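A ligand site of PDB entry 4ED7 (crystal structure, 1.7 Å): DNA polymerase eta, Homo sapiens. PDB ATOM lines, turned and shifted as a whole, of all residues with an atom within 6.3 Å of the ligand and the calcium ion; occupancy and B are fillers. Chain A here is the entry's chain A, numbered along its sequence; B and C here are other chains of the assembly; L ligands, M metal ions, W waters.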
ATOM      1  N   ASP A  16     -19.913  10.921  21.225  1.00  0.00           N
ATOM      2  CA  ASP A  16     -20.923   9.864  21.110  1.00  0.00           C
ATOM      3  C   ASP A  16     -20.298   8.754  20.234  1.00  0.00           C
ATOM      4  O   ASP A  16     -20.026   8.987  19.060  1.00  0.00           O
ATOM      5  CB  ASP A  16     -22.170  10.476  20.457  1.00  0.00           C
ATOM      6  CG  ASP A  16     -23.367   9.564  20.464  1.00  0.00           C
ATOM      7  OD1 ASP A  16     -23.202   8.364  20.729  1.00  0.00           O
ATOM      8  OD2 ASP A  16     -24.483  10.045  20.195  1.00  0.00           O
ATOM      9  N   MET A  17     -20.053   7.570  20.792  1.00  0.00           N
ATOM     10  CA  MET A  17     -19.406   6.519  19.998  1.00  0.00           C
ATOM     11  C   MET A  17     -20.319   6.096  18.844  1.00  0.00           C
ATOM     12  O   MET A  17     -21.529   6.016  19.017  1.00  0.00           O
ATOM     13  CB  MET A  17     -19.068   5.284  20.866  1.00  0.00           C
ATOM     14  CG  MET A  17     -18.234   5.592  22.114  1.00  0.00           C
ATOM     15  SD  MET A  17     -16.704   6.526  21.780  1.00  0.00           S
ATOM     16  CE  MET A  17     -15.852   5.358  20.741  1.00  0.00           C
ATOM     17  N   ASP A  18     -19.764   5.840  17.677  1.00  0.00           N
ATOM     18  CA  ASP A  18     -20.584   5.335  16.578  1.00  0.00           C
ATOM     19  C   ASP A  18     -20.977   3.882  16.795  1.00  0.00           C
ATOM     20  O   ASP A  18     -20.170   3.085  17.278  1.00  0.00           O
ATOM     21  CB  ASP A  18     -19.854   5.485  15.247  1.00  0.00           C
ATOM     22  CG  ASP A  18     -19.504   6.938  14.950  1.00  0.00           C
ATOM     23  OD1 ASP A  18     -20.264   7.831  15.358  1.00  0.00           O
ATOM     24  OD2 ASP A  18     -18.477   7.168  14.302  1.00  0.00           O
ATOM     25  N   CYS A  19     -22.221   3.547  16.432  1.00  0.00           N
ATOM     26  CA  CYS A  19     -22.764   2.192  16.590  1.00  0.00           C
ATOM     27  C   CYS A  19     -21.983   1.353  17.608  1.00  0.00           C
ATOM     28  O   CYS A  19     -21.369   0.347  17.265  1.00  0.00           O
ATOM     29  CB  CYS A  19     -22.862   1.476  15.234  1.00  0.00           C
ATOM     30  SG  CYS A  19     -21.322   1.412  14.259  1.00  0.00           S
ATOM     31  N   PHE A  20     -22.034   1.769  18.877  1.00  0.00           N
ATOM     32  CA  PHE A  20     -21.046   1.334  19.868  1.00  0.00           C
ATOM     33  C   PHE A  20     -20.909  -0.179  20.046  1.00  0.00           C
ATOM     34  O   PHE A  20     -19.816  -0.711  19.934  1.00  0.00           O
ATOM     35  CB  PHE A  20     -21.336   1.963  21.228  1.00  0.00           C
ATOM     36  CG  PHE A  20     -20.257   1.701  22.248  1.00  0.00           C
ATOM     37  CD1 PHE A  20     -18.930   1.912  21.931  1.00  0.00           C
ATOM     38  CD2 PHE A  20     -20.583   1.253  23.521  1.00  0.00           C
ATOM     39  CE1 PHE A  20     -17.926   1.677  22.873  1.00  0.00           C
ATOM     40  CE2 PHE A  20     -19.579   1.018  24.463  1.00  0.00           C
ATOM     41  CZ  PHE A  20     -18.267   1.234  24.130  1.00  0.00           C
ATOM     42  N   PHE A  21     -22.008  -0.860  20.352  1.00  0.00           N
ATOM     43  CA  PHE A  21     -21.886  -2.296  20.654  1.00  0.00           C
ATOM     44  C   PHE A  21     -21.364  -3.045  19.425  1.00  0.00           C
ATOM     45  O   PHE A  21     -20.660  -4.031  19.545  1.00  0.00           O
ATOM     46  CB  PHE A  21     -23.207  -2.916  21.131  1.00  0.00           C
ATOM     47  CG  PHE A  21     -23.623  -2.523  22.531  1.00  0.00           C
ATOM     48  CD1 PHE A  21     -23.065  -1.429  23.152  1.00  0.00           C
ATOM     49  CD2 PHE A  21     -24.566  -3.263  23.205  1.00  0.00           C
ATOM     50  CE1 PHE A  21     -23.455  -1.076  24.437  1.00  0.00           C
ATOM     51  CE2 PHE A  21     -24.964  -2.914  24.496  1.00  0.00           C
ATOM     52  CZ  PHE A  21     -24.404  -1.816  25.103  1.00  0.00           C
ATOM     53  N   VAL A  22     -21.764  -2.583  18.248  1.00  0.00           N
ATOM     54  CA  VAL A  22     -21.254  -3.140  17.001  1.00  0.00           C
ATOM     55  C   VAL A  22     -19.726  -2.998  16.895  1.00  0.00           C
ATOM     56  O   VAL A  22     -19.043  -3.957  16.572  1.00  0.00           O
ATOM     57  CB  VAL A  22     -21.940  -2.508  15.775  1.00  0.00           C
ATOM     58  CG1 VAL A  22     -21.169  -2.813  14.497  1.00  0.00           C
ATOM     59  CG2 VAL A  22     -23.399  -2.986  15.678  1.00  0.00           C
ATOM     60  N   GLN A  41     -29.770  -9.594  21.116  1.00  0.00           N
ATOM     61  CA  GLN A  41     -29.848 -10.350  22.358  1.00  0.00           C
ATOM     62  C   GLN A  41     -30.953 -11.399  22.311  1.00  0.00           C
ATOM     63  O   GLN A  41     -32.049 -11.137  21.801  1.00  0.00           O
ATOM     64  CB  GLN A  41     -29.951  -9.442  23.609  1.00  0.00           C
ATOM     65  CG  GLN A  41     -31.012  -8.376  23.572  1.00  0.00           C
ATOM     66  CD  GLN A  41     -30.928  -7.428  24.771  1.00  0.00           C
ATOM     67  OE1 GLN A  41     -29.891  -7.318  25.435  1.00  0.00           O
ATOM     68  NE2 GLN A  41     -32.021  -6.731  25.029  1.00  0.00           N
ATOM     69  N   ILE A  51     -30.123  -4.639  18.992  1.00  0.00           N
ATOM     70  CA  ILE A  51     -29.886  -3.493  19.869  1.00  0.00           C
ATOM     71  C   ILE A  51     -28.859  -2.499  19.344  1.00  0.00           C
ATOM     72  O   ILE A  51     -28.756  -1.387  19.858  1.00  0.00           O
ATOM     73  CB  ILE A  51     -29.546  -3.909  21.312  1.00  0.00           C
ATOM     74  CG1 ILE A  51     -28.270  -4.732  21.360  1.00  0.00           C
ATOM     75  CG2 ILE A  51     -30.701  -4.709  21.912  1.00  0.00           C
ATOM     76  CD1 ILE A  51     -27.807  -4.997  22.780  1.00  0.00           C
ATOM     77  N   ALA A  52     -28.089  -2.899  18.323  1.00  0.00           N
ATOM     78  CA  ALA A  52     -27.152  -1.991  17.655  1.00  0.00           C
ATOM     79  C   ALA A  52     -26.945  -2.410  16.197  1.00  0.00           C
ATOM     80  O   ALA A  52     -27.000  -3.604  15.884  1.00  0.00           O
ATOM     81  CB  ALA A  52     -25.816  -1.947  18.400  1.00  0.00           C
ATOM     82  N   VAL A  53     -26.681  -1.444  15.336  1.00  0.00           N
ATOM     83  CA  VAL A  53     -26.633  -1.688  13.893  1.00  0.00           C
ATOM     84  C   VAL A  53     -25.516  -0.906  13.188  1.00  0.00           C
ATOM     85  O   VAL A  53     -25.411   0.312  13.360  1.00  0.00           O
ATOM     86  CB  VAL A  53     -27.990  -1.274  13.239  1.00  0.00           C
ATOM     87  CG1 VAL A  53     -28.025  -1.725  11.804  1.00  0.00           C
ATOM     88  CG2 VAL A  53     -29.146  -1.866  14.002  1.00  0.00           C
ATOM     89  N   TYR A  55     -23.461   0.995  10.217  1.00  0.00           N
ATOM     90  CA  TYR A  55     -23.942   1.928   9.211  1.00  0.00           C
ATOM     91  C   TYR A  55     -24.186   1.233   7.869  1.00  0.00           C
ATOM     92  O   TYR A  55     -25.111   1.583   7.154  1.00  0.00           O
ATOM     93  CB  TYR A  55     -23.031   3.155   9.115  1.00  0.00           C
ATOM     94  CG  TYR A  55     -23.295   4.101  10.278  1.00  0.00           C
ATOM     95  CD1 TYR A  55     -22.759   3.841  11.535  1.00  0.00           C
ATOM     96  CD2 TYR A  55     -24.121   5.197  10.128  1.00  0.00           C
ATOM     97  CE1 TYR A  55     -23.021   4.686  12.610  1.00  0.00           C
ATOM     98  CE2 TYR A  55     -24.382   6.033  11.180  1.00  0.00           C
ATOM     99  CZ  TYR A  55     -23.842   5.790  12.419  1.00  0.00           C
ATOM    100  OH  TYR A  55     -24.129   6.647  13.471  1.00  0.00           O
ATOM    101  N   ARG A  58     -27.575  -0.226   8.265  1.00  0.00           N
ATOM    102  CA  ARG A  58     -28.624   0.793   8.277  1.00  0.00           C
ATOM    103  C   ARG A  58     -29.068   1.171   6.870  1.00  0.00           C
ATOM    104  O   ARG A  58     -30.241   1.509   6.665  1.00  0.00           O
ATOM    105  CB  ARG A  58     -28.175   2.051   9.027  1.00  0.00           C
ATOM    106  CG  ARG A  58     -27.844   1.779  10.471  1.00  0.00           C
ATOM    107  CD  ARG A  58     -27.370   3.047  11.168  1.00  0.00           C
ATOM    108  NE  ARG A  58     -26.768   2.683  12.440  1.00  0.00           N
ATOM    109  CZ  ARG A  58     -26.553   3.525  13.438  1.00  0.00           C
ATOM    110  NH1 ARG A  58     -26.913   4.801  13.336  1.00  0.00           N
ATOM    111  NH2 ARG A  58     -25.988   3.070  14.560  1.00  0.00           N
ATOM    112  N   ARG A  64     -32.628  -0.637  15.280  1.00  0.00           N
ATOM    113  CA  ARG A  64     -32.817  -1.126  16.644  1.00  0.00           C
ATOM    114  C   ARG A  64     -34.290  -1.466  16.897  1.00  0.00           C
ATOM    115  O   ARG A  64     -35.177  -0.860  16.309  1.00  0.00           O
ATOM    116  CB  ARG A  64     -32.318  -0.069  17.628  1.00  0.00           C
ATOM    117  CG  ARG A  64     -32.809  -0.204  19.048  1.00  0.00           C
ATOM    118  CD  ARG A  64     -32.129   0.867  19.907  1.00  0.00           C
ATOM    119  NE  ARG A  64     -30.680   0.737  19.796  1.00  0.00           N
ATOM    120  CZ  ARG A  64     -29.834   1.738  19.582  1.00  0.00           C
ATOM    121  NH1 ARG A  64     -30.285   2.989  19.469  1.00  0.00           N
ATOM    122  NH2 ARG A  64     -28.538   1.488  19.481  1.00  0.00           N
ATOM    123  N   SER A 116     -24.094   8.372  29.280  1.00  0.00           N
ATOM    124  CA  SER A 116     -24.648   7.057  29.021  1.00  0.00           C
ATOM    125  C   SER A 116     -23.486   6.103  28.820  1.00  0.00           C
ATOM    126  O   SER A 116     -22.343   6.489  28.997  1.00  0.00           O
ATOM    127  CB  SER A 116     -25.474   7.079  27.751  1.00  0.00           C
ATOM    128  OG  SER A 116     -24.611   7.170  26.624  1.00  0.00           O
ATOM    129  N   ILE A 117     -23.768   4.865  28.427  1.00  0.00           N
ATOM    130  CA  ILE A 117     -22.698   3.893  28.238  1.00  0.00           C
ATOM    131  C   ILE A 117     -21.693   4.330  27.170  1.00  0.00           C
ATOM    132  O   ILE A 117     -20.539   3.916  27.189  1.00  0.00           O
ATOM    133  CB  ILE A 117     -23.243   2.491  27.896  1.00  0.00           C
ATOM    134  CG1 ILE A 117     -22.131   1.442  28.017  1.00  0.00           C
ATOM    135  CG2 ILE A 117     -23.862   2.481  26.517  1.00  0.00           C
ATOM    136  CD1 ILE A 117     -22.656   0.010  28.132  1.00  0.00           C
ATOM    137  N   ASP A 118     -22.105   5.189  26.231  1.00  0.00           N
ATOM    138  CA  ASP A 118     -21.171   5.541  25.164  1.00  0.00           C
ATOM    139  C   ASP A 118     -21.151   7.037  24.822  1.00  0.00           C
ATOM    140  O   ASP A 118     -20.737   7.428  23.733  1.00  0.00           O
ATOM    141  CB  ASP A 118     -21.455   4.718  23.920  1.00  0.00           C
ATOM    142  CG  ASP A 118     -22.594   5.273  23.116  1.00  0.00           C
ATOM    143  OD1 ASP A 118     -22.534   5.122  21.885  1.00  0.00           O
ATOM    144  OD2 ASP A 118     -23.509   5.883  23.709  1.00  0.00           O
ATOM    145  N   GLU A 119     -21.622   7.867  25.755  1.00  0.00           N
ATOM    146  CA  GLU A 119     -21.623   9.319  25.554  1.00  0.00           C
ATOM    147  C   GLU A 119     -21.056  10.012  26.782  1.00  0.00           C
ATOM    148  O   GLU A 119     -21.340   9.618  27.912  1.00  0.00           O
ATOM    149  CB  GLU A 119     -23.039   9.847  25.340  1.00  0.00           C
ATOM    150  CG  GLU A 119     -23.767   9.209  24.152  1.00  0.00           C
ATOM    151  CD  GLU A 119     -25.148   9.813  23.938  1.00  0.00           C
ATOM    152  OE1 GLU A 119     -25.837  10.101  24.932  1.00  0.00           O
ATOM    153  OE2 GLU A 119     -25.526  10.010  22.764  1.00  0.00           O
ATOM    154  N   LYS A 227     -24.959  18.306  21.987  1.00  0.00           N
ATOM    155  CA  LYS A 227     -25.648  17.064  21.666  1.00  0.00           C
ATOM    156  C   LYS A 227     -26.317  17.162  20.297  1.00  0.00           C
ATOM    157  O   LYS A 227     -26.197  16.262  19.474  1.00  0.00           O
ATOM    158  CB  LYS A 227     -26.691  16.742  22.746  1.00  0.00           C
ATOM    159  CG  LYS A 227     -27.576  15.539  22.442  1.00  0.00           C
ATOM    160  CD  LYS A 227     -26.756  14.277  22.189  1.00  0.00           C
ATOM    161  CE  LYS A 227     -27.664  13.085  21.884  1.00  0.00           C
ATOM    162  NZ  LYS A 227     -26.886  11.882  21.456  1.00  0.00           N
ATOM    163  N   LYS A 234     -22.923  12.287  11.496  1.00  0.00           N
ATOM    164  CA  LYS A 234     -22.446  10.974  11.914  1.00  0.00           C
ATOM    165  C   LYS A 234     -22.362  10.102  10.668  1.00  0.00           C
ATOM    166  O   LYS A 234     -23.089  10.319   9.703  1.00  0.00           O
ATOM    167  CB  LYS A 234     -23.434  10.339  12.904  1.00  0.00           C
ATOM    168  CG  LYS A 234     -23.219  10.689  14.378  1.00  0.00           C
ATOM    169  CD  LYS A 234     -23.867   9.608  15.283  1.00  0.00           C
ATOM    170  CE  LYS A 234     -23.319   9.628  16.727  1.00  0.00           C
ATOM    171  NZ  LYS A 234     -22.325   8.522  17.038  1.00  0.00           N
ATOM    172  N   PRO A 235     -21.459   9.102  10.682  1.00  0.00           N
ATOM    173  CA  PRO A 235     -20.524   8.777  11.755  1.00  0.00           C
ATOM    174  C   PRO A 235     -19.132   9.355  11.527  1.00  0.00           C
ATOM    175  O   PRO A 235     -18.853   9.888  10.456  1.00  0.00           O
ATOM    176  CB  PRO A 235     -20.447   7.255  11.674  1.00  0.00           C
ATOM    177  CG  PRO A 235     -20.551   6.990  10.197  1.00  0.00           C
ATOM    178  CD  PRO A 235     -21.490   8.044   9.649  1.00  0.00           C
ATOM    179  P    DT B   3     -43.485  -6.946  21.259  1.00  0.00           P
ATOM    180  OP1  DT B   3     -44.940  -6.872  21.503  1.00  0.00           O
ATOM    181  OP2  DT B   3     -42.947  -6.726  19.901  1.00  0.00           O
ATOM    182  O5'  DT B   3     -42.761  -5.917  22.255  1.00  0.00           O
ATOM    183  C5'  DT B   3     -41.536  -5.307  21.886  1.00  0.00           C
ATOM    184  C4'  DT B   3     -40.361  -6.177  22.290  1.00  0.00           C
ATOM    185  O4'  DT B   3     -39.149  -5.655  21.673  1.00  0.00           O
ATOM    186  C3'  DT B   3     -40.086  -6.257  23.789  1.00  0.00           C
ATOM    187  O3'  DT B   3     -39.860  -7.620  24.144  1.00  0.00           O
ATOM    188  C2'  DT B   3     -38.850  -5.400  23.995  1.00  0.00           C
ATOM    189  C1'  DT B   3     -38.136  -5.533  22.658  1.00  0.00           C
ATOM    190  N1   DT B   3     -37.298  -4.351  22.270  1.00  0.00           N
ATOM    191  C2   DT B   3     -35.962  -4.528  21.965  1.00  0.00           C
ATOM    192  O2   DT B   3     -35.396  -5.613  21.999  1.00  0.00           O
ATOM    193  N3   DT B   3     -35.302  -3.370  21.619  1.00  0.00           N
ATOM    194  C4   DT B   3     -35.831  -2.099  21.550  1.00  0.00           C
ATOM    195  O4   DT B   3     -35.159  -1.122  21.233  1.00  0.00           O
ATOM    196  C5   DT B   3     -37.237  -1.987  21.876  1.00  0.00           C
ATOM    197  C7   DT B   3     -37.926  -0.658  21.833  1.00  0.00           C
ATOM    198  C6   DT B   3     -37.890  -3.105  22.209  1.00  0.00           C
ATOM    199  P    DT B   4     -39.464  -8.003  25.653  1.00  0.00           P
ATOM    200  OP1  DT B   4     -39.497  -9.475  25.772  1.00  0.00           O
ATOM    201  OP2  DT B   4     -40.297  -7.185  26.560  1.00  0.00           O
ATOM    202  O5'  DT B   4     -37.944  -7.483  25.775  1.00  0.00           O
ATOM    203  C5'  DT B   4     -36.903  -8.242  25.182  1.00  0.00           C
ATOM    204  C4'  DT B   4     -35.603  -7.900  25.877  1.00  0.00           C
ATOM    205  O4'  DT B   4     -35.139  -6.623  25.390  1.00  0.00           O
ATOM    206  C3'  DT B   4     -35.700  -7.774  27.396  1.00  0.00           C
ATOM    207  O3'  DT B   4     -34.538  -8.421  27.883  1.00  0.00           O
ATOM    208  C2'  DT B   4     -35.709  -6.271  27.629  1.00  0.00           C
ATOM    209  C1'  DT B   4     -34.823  -5.785  26.482  1.00  0.00           C
ATOM    210  N1   DT B   4     -35.071  -4.413  25.972  1.00  0.00           N
ATOM    211  C2   DT B   4     -33.968  -3.693  25.573  1.00  0.00           C
ATOM    212  O2   DT B   4     -32.843  -4.143  25.652  1.00  0.00           O
ATOM    213  N3   DT B   4     -34.242  -2.443  25.090  1.00  0.00           N
ATOM    214  C4   DT B   4     -35.469  -1.847  24.963  1.00  0.00           C
ATOM    215  O4   DT B   4     -35.599  -0.717  24.511  1.00  0.00           O
ATOM    216  C5   DT B   4     -36.594  -2.651  25.391  1.00  0.00           C
ATOM    217  C7   DT B   4     -37.990  -2.107  25.294  1.00  0.00           C
ATOM    218  C6   DT B   4     -36.344  -3.879  25.860  1.00  0.00           C
ATOM    219  P    DA B   5     -34.177  -8.430  29.447  1.00  0.00           P
ATOM    220  OP1  DA B   5     -33.574  -9.728  29.762  1.00  0.00           O
ATOM    221  OP2  DA B   5     -35.355  -7.939  30.188  1.00  0.00           O
ATOM    222  O5'  DA B   5     -33.063  -7.283  29.575  1.00  0.00           O
ATOM    223  C5'  DA B   5     -31.793  -7.440  28.949  1.00  0.00           C
ATOM    224  C4'  DA B   5     -30.908  -6.269  29.319  1.00  0.00           C
ATOM    225  O4'  DA B   5     -31.371  -5.071  28.630  1.00  0.00           O
ATOM    226  C3'  DA B   5     -30.889  -5.925  30.808  1.00  0.00           C
ATOM    227  O3'  DA B   5     -29.552  -5.616  31.143  1.00  0.00           O
ATOM    228  C2'  DA B   5     -31.780  -4.690  30.884  1.00  0.00           C
ATOM    229  C1'  DA B   5     -31.446  -4.011  29.560  1.00  0.00           C
ATOM    230  N9   DA B   5     -32.441  -3.044  29.087  1.00  0.00           N
ATOM    231  C8   DA B   5     -33.800  -3.135  29.163  1.00  0.00           C
ATOM    232  N7   DA B   5     -34.435  -2.112  28.637  1.00  0.00           N
ATOM    233  C5   DA B   5     -33.422  -1.283  28.175  1.00  0.00           C
ATOM    234  C6   DA B   5     -33.441  -0.031  27.526  1.00  0.00           C
ATOM    235  N6   DA B   5     -34.583   0.615  27.217  1.00  0.00           N
ATOM    236  N1   DA B   5     -32.264   0.525  27.197  1.00  0.00           N
ATOM    237  C2   DA B   5     -31.130  -0.125  27.511  1.00  0.00           C
ATOM    238  N3   DA B   5     -30.984  -1.304  28.129  1.00  0.00           N
ATOM    239  C4   DA B   5     -32.192  -1.839  28.437  1.00  0.00           C
ATOM    240  P    DT C   8     -30.863   9.305  23.262  1.00  0.00           P
ATOM    241  OP1  DT C   8     -29.968  10.071  22.375  1.00  0.00           O
ATOM    242  OP2  DT C   8     -31.971   8.528  22.653  1.00  0.00           O
ATOM    243  O5'  DT C   8     -29.970   8.281  24.154  1.00  0.00           O
ATOM    244  C5'  DT C   8     -28.644   8.571  24.665  1.00  0.00           C
ATOM    245  C4'  DT C   8     -27.954   7.337  25.270  1.00  0.00           C
ATOM    246  O4'  DT C   8     -28.981   6.606  25.970  1.00  0.00           O
ATOM    247  C3'  DT C   8     -27.348   6.377  24.234  1.00  0.00           C
ATOM    248  O3'  DT C   8     -26.065   5.995  24.701  1.00  0.00           O
ATOM    249  C2'  DT C   8     -28.270   5.158  24.228  1.00  0.00           C
ATOM    250  C1'  DT C   8     -28.893   5.232  25.616  1.00  0.00           C
ATOM    251  N1   DT C   8     -30.280   4.706  25.651  1.00  0.00           N
ATOM    252  C2   DT C   8     -30.487   3.449  26.179  1.00  0.00           C
ATOM    253  O2   DT C   8     -29.579   2.749  26.618  1.00  0.00           O
ATOM    254  N3   DT C   8     -31.796   3.037  26.192  1.00  0.00           N
ATOM    255  C4   DT C   8     -32.885   3.748  25.707  1.00  0.00           C
ATOM    256  O4   DT C   8     -34.018   3.314  25.748  1.00  0.00           O
ATOM    257  C5   DT C   8     -32.593   5.043  25.156  1.00  0.00           C
ATOM    258  C7   DT C   8     -33.736   5.868  24.622  1.00  0.00           C
ATOM    259  C6   DT C   8     -31.320   5.456  25.153  1.00  0.00           C
HETATM  260  P1  LIG L   1     -25.076   5.762  16.825  1.00  0.00           P
HETATM  261  O1  LIG L   1     -26.342   6.229  16.152  1.00  0.00           O
HETATM  262  O2  LIG L   1     -23.906   5.604  15.892  1.00  0.00           O
HETATM  263  O3  LIG L   1     -24.767   6.516  18.080  1.00  0.00           O
HETATM  264  P2  LIG L   1     -25.357   3.535  18.658  1.00  0.00           P
HETATM  265  O4  LIG L   1     -24.086   3.955  19.343  1.00  0.00           O
HETATM  266  O5  LIG L   1     -25.577   2.069  18.415  1.00  0.00           O
HETATM  267  O6  LIG L   1     -25.476   4.235  17.215  1.00  0.00           O
HETATM  268  P3  LIG L   1     -26.812   4.801  20.830  1.00  0.00           P
HETATM  269  O7  LIG L   1     -28.265   5.194  20.939  1.00  0.00           O
HETATM  270  O8  LIG L   1     -25.810   5.902  21.011  1.00  0.00           O
HETATM  271  O9  LIG L   1     -26.666   4.118  19.378  1.00  0.00           O
HETATM  272  O10 LIG L   1     -26.566   3.645  21.928  1.00  0.00           O
HETATM  273  C1  LIG L   1     -25.275   3.219  22.329  1.00  0.00           C
HETATM  274  C2  LIG L   1     -25.347   1.758  22.708  1.00  0.00           C
HETATM  275  O11 LIG L   1     -26.316   1.552  23.743  1.00  0.00           O
HETATM  276  C3  LIG L   1     -25.848   0.946  21.522  1.00  0.00           C
HETATM  277  O12 LIG L   1     -24.794   0.546  20.636  1.00  0.00           O
HETATM  278  C4  LIG L   1     -26.536  -0.238  22.186  1.00  0.00           C
HETATM  279  C5  LIG L   1     -27.081   0.363  23.482  1.00  0.00           C
HETATM  280  N1  LIG L   1     -28.499   0.774  23.352  1.00  0.00           N
HETATM  281  C6  LIG L   1     -28.979   1.934  22.871  1.00  0.00           C
HETATM  282  N2  LIG L   1     -30.341   1.900  22.937  1.00  0.00           N
HETATM  283  C7  LIG L   1     -30.686   0.715  23.475  1.00  0.00           C
HETATM  284  C8  LIG L   1     -31.898   0.108  23.788  1.00  0.00           C
HETATM  285  N3  LIG L   1     -33.059   0.767  23.559  1.00  0.00           N
HETATM  286  N4  LIG L   1     -31.894  -1.137  24.327  1.00  0.00           N
HETATM  287  C9  LIG L   1     -30.750  -1.783  24.564  1.00  0.00           C
HETATM  288  N5  LIG L   1     -29.566  -1.230  24.279  1.00  0.00           N
HETATM  289  C10 LIG L   1     -29.517   0.022  23.741  1.00  0.00           C
HETATM  290 CA    CA M   1     -23.647   6.155  20.057  1.00  0.00          CA
HETATM  291  O   HOH W   1     -26.947   1.066  16.490  1.00  0.00           O
HETATM  292  O   HOH W   2     -32.300   3.597  22.089  1.00  0.00           O
HETATM  293  O   HOH W   3     -29.832   6.515  18.808  1.00  0.00           O
HETATM  294  O   HOH W   4     -27.235   1.869  26.428  1.00  0.00           O
HETATM  295  O   HOH W   5     -27.824  -2.549  26.099  1.00  0.00           O
HETATM  296  O   HOH W   6     -28.856   5.224  16.328  1.00  0.00           O
HETATM  297  O   HOH W   7     -30.869   5.965  21.879  1.00  0.00           O
HETATM  298  O   HOH W   8     -26.548   8.456  20.235  1.00  0.00           O
HETATM  299  O   HOH W   9     -27.301   8.457  17.583  1.00  0.00           O
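Water W2 lies within hydrogen-bond range of a nitrogen (N2) of the ligand and the guanidinium group (NH1) of Arg 64. Water W8 bridges the side-chain carboxylate of Asp 16 (2.6 Å) and the side-chain carboxylate of Glu 119 (3.1 Å). Water W4 lies within hydrogen-bond range of O2 of DT 8 of chain C (2.5 Å) and an oxygen (O11) of the ligand (2.9 Å). Water W7 bridges O7 of the ligand (2.9 Å) and OP2 of DT 8 of chain C (2.9 Å).
The side-chain hydroxyl (OH) of Tyr 55 sits at hydrogen-bond distance from an oxygen (O2) of the ligand (2.6 Å). The backbone NH of Cys 19 lies within hydrogen-bond range of an oxygen (O2) of the ligand, at 2.7 Å. N3 of the ligand lies within hydrogen-bond range of O4 of DT 4 of chain B. An oxygen (O1) of the ligand lies within salt-bridge range of the guanidinium group (NH1) of Arg 58 (3.2 Å). The backbone NH (N) of Phe 20 is in hydrogen-bond range of an oxygen (O12) of the ligand. The backbone NH (N) of Phe 21 is in hydrogen-bond range of an oxygen (O12) of the ligand (3.1 Å). NH2 of Arg 64 is in salt-bridge range of O5 of the ligand. O4 of DT 8 of chain C is in hydrogen-bond range of a nitrogen (N3) of the ligand. The side-chain amino group of Lys 234 lies within salt-bridge range of an oxygen (O2) of the ligand (3.5 Å).
O3 of the ligand binds the calcium ion. OD1 of Asp 16 binds the calcium ion (2.4 Å). The calcium ion is bound by O4 of the ligand, 2.4 Å away. O of Met 17 is bound to the calcium ion (2.4 Å). The calcium ion is bound by OD1 of Asp 118 (2.4 Å). An oxygen (O8) of the ligand is bound to the calcium ion (2.4 Å). The calcium ion has six donor atoms within binding distance.
Of the 25 residues printed, 3 come within 4 Å of the calcium ion. Along chain A the residues within 4 Å of the calcium ion span positions 16 to 118.
The backbone carbonyl oxygen of Met 17 lies close to the side-chain amino group of Lys 234, at 3.3 Å. OD2 of Asp 118 sits close to O3' of DT 8 of chain C. The side-chain hydroxyl of Ser 116 lies close to the backbone NH of Asp 118 (3.2 Å). The side-chain hydroxyl (OH) of Tyr 55 sits at hydrogen-bond distance from the guanidinium group (NH1) of Arg 58 (3.3 Å). O2 of DT 4 of chain B sits at hydrogen-bond distance from the side-chain amide nitrogen of Gln 41 (2.8 Å). The guanidinium group (NE) of Arg 58 is in hydrogen-bond range of the backbone carbonyl oxygen (O) of Val 53, 2.9 Å away. NE of Arg 64 is in hydrogen-bond range of O of Ile 51 (2.9 Å). N1 of DA 5 of chain B sits close to N3 of DT 8 of chain C (2.7 Å).
A nitrogen (N4) of the ligand lies close to N1 of DA 5 of chain B, at 3.3 Å. CA of Asp 18 touches O2 of the ligand, 3.4 Å away. O of Ile 51 touches C4 of the ligand (3.4 Å). Ala 52 touches the ligand (CB to O12, 3.5 Å). CG2 of Ile 117 touches O11 of the ligand (3.8 Å). DT 3 of chain B touches the ligand (O4 to N3, 3.7 Å). Hydrophobic or aromatic side chains that line the ligand: Phe 20, Phe 21, Ile 51, Ala 52, Tyr 55 and Ile 117. Within 4 Å of the ligand: Asp 16, Met 17, Asp 18, Cys 19, Phe 20, Phe 21, Ile 51, Ala 52, Tyr 55, Arg 58, Arg 64, Ile 117, Asp 118, Lys 234, DT 3 of chain B, DT 4 of chain B, DA 5 of chain B and DT 8 of chain C. Along chain A the residues within 4 Å of the ligand span positions 16 to 234.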
